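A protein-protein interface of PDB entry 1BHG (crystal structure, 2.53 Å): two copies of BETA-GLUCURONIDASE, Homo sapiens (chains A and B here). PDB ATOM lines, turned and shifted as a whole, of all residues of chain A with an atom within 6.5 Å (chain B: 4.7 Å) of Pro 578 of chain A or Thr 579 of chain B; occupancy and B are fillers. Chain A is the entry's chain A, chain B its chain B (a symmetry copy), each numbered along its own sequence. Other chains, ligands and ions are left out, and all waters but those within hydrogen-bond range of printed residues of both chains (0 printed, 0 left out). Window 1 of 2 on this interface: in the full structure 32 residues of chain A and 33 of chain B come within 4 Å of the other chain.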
ATOM      1  N   TYR A 491       2.601   5.235  24.408  1.00  0.00           N
ATOM      2  CA  TYR A 491       2.057   6.145  23.440  1.00  0.00           C
ATOM      3  C   TYR A 491       2.805   7.484  23.344  1.00  0.00           C
ATOM      4  O   TYR A 491       2.832   8.260  24.307  1.00  0.00           O
ATOM      5  CB  TYR A 491       0.610   6.387  23.803  1.00  0.00           C
ATOM      6  CG  TYR A 491      -0.200   5.154  24.013  1.00  0.00           C
ATOM      7  CD1 TYR A 491       0.098   3.957  23.350  1.00  0.00           C
ATOM      8  CD2 TYR A 491      -1.370   5.214  24.777  1.00  0.00           C
ATOM      9  CE1 TYR A 491      -0.772   2.854  23.432  1.00  0.00           C
ATOM     10  CE2 TYR A 491      -2.249   4.131  24.866  1.00  0.00           C
ATOM     11  CZ  TYR A 491      -1.957   2.962  24.189  1.00  0.00           C
ATOM     12  OH  TYR A 491      -2.911   1.954  24.213  1.00  0.00           O
ATOM     13  N   PHE A 537      -0.969  10.269  14.755  1.00  0.00           N
ATOM     14  CA  PHE A 537      -1.033   9.787  13.360  1.00  0.00           C
ATOM     15  C   PHE A 537      -0.527  10.902  12.413  1.00  0.00           C
ATOM     16  O   PHE A 537      -1.254  11.414  11.564  1.00  0.00           O
ATOM     17  CB  PHE A 537      -2.478   9.464  12.994  1.00  0.00           C
ATOM     18  CG  PHE A 537      -3.164   8.508  13.930  1.00  0.00           C
ATOM     19  CD1 PHE A 537      -3.202   8.740  15.297  1.00  0.00           C
ATOM     20  CD2 PHE A 537      -3.871   7.422  13.404  1.00  0.00           C
ATOM     21  CE1 PHE A 537      -3.936   7.912  16.117  1.00  0.00           C
ATOM     22  CE2 PHE A 537      -4.606   6.584  14.187  1.00  0.00           C
ATOM     23  CZ  PHE A 537      -4.659   6.812  15.548  1.00  0.00           C
ATOM     24  N   GLN A 576     -13.703  -2.968  10.479  1.00  0.00           N
ATOM     25  CA  GLN A 576     -13.951  -1.681  11.184  1.00  0.00           C
ATOM     26  C   GLN A 576     -13.764  -1.669  12.714  1.00  0.00           C
ATOM     27  O   GLN A 576     -14.560  -2.327  13.424  1.00  0.00           O
ATOM     28  CB  GLN A 576     -15.382  -1.167  10.936  1.00  0.00           C
ATOM     29  CG  GLN A 576     -15.751  -0.789   9.541  1.00  0.00           C
ATOM     30  CD  GLN A 576     -17.204  -0.388   9.440  1.00  0.00           C
ATOM     31  OE1 GLN A 576     -18.033  -1.110   8.898  1.00  0.00           O
ATOM     32  NE2 GLN A 576     -17.523   0.774   9.959  1.00  0.00           N
ATOM     33  N   SER A 577     -12.772  -0.920  13.221  1.00  0.00           N
ATOM     34  CA  SER A 577     -12.528  -0.774  14.671  1.00  0.00           C
ATOM     35  C   SER A 577     -12.012   0.653  14.947  1.00  0.00           C
ATOM     36  O   SER A 577     -11.422   1.245  14.051  1.00  0.00           O
ATOM     37  CB  SER A 577     -11.517  -1.787  15.192  1.00  0.00           C
ATOM     38  OG  SER A 577     -10.267  -1.695  14.549  1.00  0.00           O
ATOM     39  N   PRO A 578     -12.240   1.221  16.169  1.00  0.00           N
ATOM     40  CA  PRO A 578     -11.834   2.562  16.619  1.00  0.00           C
ATOM     41  C   PRO A 578     -10.354   2.815  16.447  1.00  0.00           C
ATOM     42  O   PRO A 578      -9.897   3.945  16.420  1.00  0.00           O
ATOM     43  CB  PRO A 578     -12.174   2.551  18.115  1.00  0.00           C
ATOM     44  CG  PRO A 578     -13.365   1.640  18.202  1.00  0.00           C
ATOM     45  CD  PRO A 578     -12.993   0.521  17.236  1.00  0.00           C
ATOM     46  N   THR A 579      -9.595   1.742  16.422  1.00  0.00           N
ATOM     47  CA  THR A 579      -8.161   1.840  16.272  1.00  0.00           C
ATOM     48  C   THR A 579      -7.765   1.790  14.796  1.00  0.00           C
ATOM     49  O   THR A 579      -6.638   2.109  14.426  1.00  0.00           O
ATOM     50  CB  THR A 579      -7.564   0.685  17.002  1.00  0.00           C
ATOM     51  OG1 THR A 579      -8.559  -0.348  17.090  1.00  0.00           O
ATOM     52  CG2 THR A 579      -7.154   1.114  18.413  1.00  0.00           C
ATOM     53  N   ARG A 580      -8.719   1.436  13.949  1.00  0.00           N
ATOM     54  CA  ARG A 580      -8.464   1.330  12.541  1.00  0.00           C
ATOM     55  C   ARG A 580      -9.271   2.395  11.807  1.00  0.00           C
ATOM     56  O   ARG A 580     -10.513   2.378  11.793  1.00  0.00           O
ATOM     57  CB  ARG A 580      -8.805  -0.084  12.083  1.00  0.00           C
ATOM     58  CG  ARG A 580      -7.785  -1.106  12.548  1.00  0.00           C
ATOM     59  CD  ARG A 580      -6.496  -0.822  11.861  1.00  0.00           C
ATOM     60  NE  ARG A 580      -5.384  -1.707  12.207  1.00  0.00           N
ATOM     61  CZ  ARG A 580      -4.706  -1.647  13.339  1.00  0.00           C
ATOM     62  NH1 ARG A 580      -5.029  -0.763  14.260  1.00  0.00           N
ATOM     63  NH2 ARG A 580      -3.615  -2.370  13.490  1.00  0.00           N
ATOM     64  N   VAL A 581      -8.553   3.340  11.200  1.00  0.00           N
ATOM     65  CA  VAL A 581      -9.220   4.434  10.509  1.00  0.00           C
ATOM     66  C   VAL A 581      -9.299   4.172   9.021  1.00  0.00           C
ATOM     67  O   VAL A 581      -8.391   4.545   8.266  1.00  0.00           O
ATOM     68  CB  VAL A 581      -8.533   5.774  10.865  1.00  0.00           C
ATOM     69  CG1 VAL A 581      -7.069   5.537  11.128  1.00  0.00           C
ATOM     70  CG2 VAL A 581      -8.781   6.856   9.793  1.00  0.00           C
ATOM     71  N   TYR B 491     -19.094  -2.285  16.544  1.00  0.00           N
ATOM     72  CA  TYR B 491     -18.511  -1.405  15.525  1.00  0.00           C
ATOM     73  C   TYR B 491     -19.133  -1.408  14.122  1.00  0.00           C
ATOM     74  O   TYR B 491     -19.177  -2.446  13.430  1.00  0.00           O
ATOM     75  CB  TYR B 491     -17.002  -1.647  15.438  1.00  0.00           C
ATOM     76  CG  TYR B 491     -16.349  -1.914  16.772  1.00  0.00           C
ATOM     77  CD1 TYR B 491     -16.861  -1.376  17.955  1.00  0.00           C
ATOM     78  CD2 TYR B 491     -15.260  -2.765  16.865  1.00  0.00           C
ATOM     79  CE1 TYR B 491     -16.307  -1.691  19.204  1.00  0.00           C
ATOM     80  CE2 TYR B 491     -14.693  -3.095  18.111  1.00  0.00           C
ATOM     81  CZ  TYR B 491     -15.225  -2.552  19.274  1.00  0.00           C
ATOM     82  OH  TYR B 491     -14.668  -2.891  20.493  1.00  0.00           O
ATOM     83  N   GLU B 524     -16.573   9.499  15.820  1.00  0.00           N
ATOM     84  CA  GLU B 524     -15.338  10.155  15.494  1.00  0.00           C
ATOM     85  C   GLU B 524     -15.301  10.321  13.968  1.00  0.00           C
ATOM     86  O   GLU B 524     -15.755   9.441  13.229  1.00  0.00           O
ATOM     87  CB  GLU B 524     -14.184   9.304  15.985  1.00  0.00           C
ATOM     88  CG  GLU B 524     -12.880   9.999  15.867  1.00  0.00           C
ATOM     89  CD  GLU B 524     -12.203  10.273  17.200  1.00  0.00           C
ATOM     90  OE1 GLU B 524     -12.923  10.250  18.252  1.00  0.00           O
ATOM     91  OE2 GLU B 524     -10.945  10.499  17.156  1.00  0.00           O
ATOM     92  N   PHE B 537     -14.389   6.519  10.450  1.00  0.00           N
ATOM     93  CA  PHE B 537     -14.241   7.955  10.650  1.00  0.00           C
ATOM     94  C   PHE B 537     -14.578   8.690   9.327  1.00  0.00           C
ATOM     95  O   PHE B 537     -13.831   9.518   8.821  1.00  0.00           O
ATOM     96  CB  PHE B 537     -12.803   8.278  11.048  1.00  0.00           C
ATOM     97  CG  PHE B 537     -12.291   7.510  12.239  1.00  0.00           C
ATOM     98  CD1 PHE B 537     -12.346   6.132  12.282  1.00  0.00           C
ATOM     99  CD2 PHE B 537     -11.685   8.175  13.285  1.00  0.00           C
ATOM    100  CE1 PHE B 537     -11.804   5.429  13.374  1.00  0.00           C
ATOM    101  CE2 PHE B 537     -11.152   7.486  14.354  1.00  0.00           C
ATOM    102  CZ  PHE B 537     -11.203   6.118  14.400  1.00  0.00           C
ATOM    103  N   SER B 577      -3.237   8.398  22.116  1.00  0.00           N
ATOM    104  CA  SER B 577      -3.726   7.021  22.084  1.00  0.00           C
ATOM    105  C   SER B 577      -4.044   6.566  20.627  1.00  0.00           C
ATOM    106  O   SER B 577      -4.646   7.331  19.840  1.00  0.00           O
ATOM    107  CB  SER B 577      -5.005   6.927  22.908  1.00  0.00           C
ATOM    108  OG  SER B 577      -4.801   7.547  24.167  1.00  0.00           O
ATOM    109  N   PRO B 578      -3.714   5.294  20.278  1.00  0.00           N
ATOM    110  CA  PRO B 578      -3.969   4.752  18.945  1.00  0.00           C
ATOM    111  C   PRO B 578      -5.461   4.868  18.545  1.00  0.00           C
ATOM    112  O   PRO B 578      -5.823   4.792  17.387  1.00  0.00           O
ATOM    113  CB  PRO B 578      -3.499   3.304  19.085  1.00  0.00           C
ATOM    114  CG  PRO B 578      -2.422   3.377  20.116  1.00  0.00           C
ATOM    115  CD  PRO B 578      -3.043   4.279  21.120  1.00  0.00           C
ATOM    116  N   THR B 579      -6.295   5.154  19.526  1.00  0.00           N
ATOM    117  CA  THR B 579      -7.735   5.329  19.349  1.00  0.00           C
ATOM    118  C   THR B 579      -8.071   6.807  18.991  1.00  0.00           C
ATOM    119  O   THR B 579      -9.114   7.092  18.380  1.00  0.00           O
ATOM    120  CB  THR B 579      -8.413   4.965  20.695  1.00  0.00           C
ATOM    121  OG1 THR B 579      -7.678   3.878  21.287  1.00  0.00           O
ATOM    122  CG2 THR B 579      -9.892   4.555  20.513  1.00  0.00           C
ATOM    123  N   ARG B 580      -7.173   7.722  19.396  1.00  0.00           N
ATOM    124  CA  ARG B 580      -7.292   9.177  19.206  1.00  0.00           C
ATOM    125  C   ARG B 580      -6.380   9.686  18.110  1.00  0.00           C
ATOM    126  O   ARG B 580      -5.155   9.693  18.276  1.00  0.00           O
ATOM    127  CB  ARG B 580      -6.942   9.927  20.510  1.00  0.00           C
ATOM    128  CG  ARG B 580      -8.027   9.980  21.579  1.00  0.00           C
ATOM    129  CD  ARG B 580      -9.418  10.100  20.991  1.00  0.00           C
ATOM    130  NE  ARG B 580     -10.459  10.160  22.030  1.00  0.00           N
ATOM    131  CZ  ARG B 580     -11.614   9.492  22.009  1.00  0.00           C
ATOM    132  NH1 ARG B 580     -11.907   8.682  21.009  1.00  0.00           N
ATOM    133  NH2 ARG B 580     -12.505   9.679  22.966  1.00  0.00           N
ATOM    134  N   VAL B 581      -6.993  10.229  17.054  1.00  0.00           N
ATOM    135  CA  VAL B 581      -6.224  10.704  15.910  1.00  0.00           C
ATOM    136  C   VAL B 581      -5.335  11.917  16.187  1.00  0.00           C
ATOM    137  O   VAL B 581      -4.125  11.805  16.150  1.00  0.00           O
ATOM    138  CB  VAL B 581      -7.121  10.833  14.648  1.00  0.00           C
ATOM    139  CG1 VAL B 581      -6.246  11.003  13.387  1.00  0.00           C
ATOM    140  CG2 VAL B 581      -7.964   9.540  14.496  1.00  0.00           C
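The side-chain hydroxyl (OG1) of Thr 579 of chain A lies within hydrogen-bond range of the side-chain hydroxyl (OG) of Ser 577 of chain A, at 3.3 Å. The side-chain carboxylate (OE1) of Glu 524 of chain B is in salt-bridge range of the guanidinium group (NH1) of Arg 580 of chain B (3.3 Å).
CZ of Tyr 491 of chain A touches CD of Pro 578 of chain B, 3.5 Å away. Phe 537 of chain A touches Ser 577 of chain B (CE1 to O, 3.8 Å). Pro 578 of chain B touches Phe 537 of chain A. CE1 of Phe 537 of chain A touches O of Arg 580 of chain B, 3.1 Å away. Phe 537 of chain A touches Val 581 of chain B (CD1 to O, 3.3 Å). Phe 537 of chain B touches Pro 578 of chain A (CZ to O, 3.2 Å). O of Pro 578 of chain A touches O of Thr 579 of chain B (3.8 Å). O of Pro 578 of chain B touches CA of Thr 579 of chain A, at 3.9 Å. Arg 580 of chain A touches Phe 537 of chain B. Phe 537 of chain B touches Val 581 of chain A.
Printed residues of chain B within 4 Å of Pro 578 of chain A: Phe 537 and Thr 579. Thr 579 of chain B touches just one residue of chain A: Pro 578. Of the printed residues of chain B, Arg 580 of chain A touches Phe 537. Of the printed residues of chain B, Val 581 of chain A touches Phe 537. Printed residues of chain B within 4 Å of Gln 576 of chain A: Tyr 491 (3.2 Å). Of the printed residues of chain B, Thr 579 of chain A touches Pro 578 (3.9 Å). Of the printed residues of chain A, Ser 577 of chain B touches Phe 537 (3.8 Å). The nearest printed residue of chain B that does not touch Pro 578 of chain A is Tyr 491 of chain B (4.01 Å). The nearest residue of chain A that does not touch Thr 579 of chain B is Thr 579 of chain A (4.02 Å). The nearest printed residue of chain A that does not touch Val 581 of chain B is Val 581 of chain A (5.3 Å).
Of the 8 printed residues of chain A, 7 touch a printed residue of chain B. Hydrophobic or aromatic side chains of chain B within 4 Å of the printed part of chain A: Tyr 491, Phe 537 and Pro 578.
Phe 537 of chain A touches Ser 577 of chain B, but with the chains exchanged Ser 577 of chain A does not touch Phe 537 of chain B (4.3 Å). Phe 537 of chain A touches Arg 580 of chain B, and with the chains exchanged Arg 580 of chain A touches Phe 537 of chain B. Phe 537 of chain A touches Val 581 of chain B, and with the chains exchanged Val 581 of chain A touches Phe 537 of chain B. Pro 578 of chain A touches Thr 579 of chain B, and with the chains exchanged Thr 579 of chain A touches Pro 578 of chain B. Positions printed for both chains: 491, 537, 577, 578, 579, 580 and 581.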
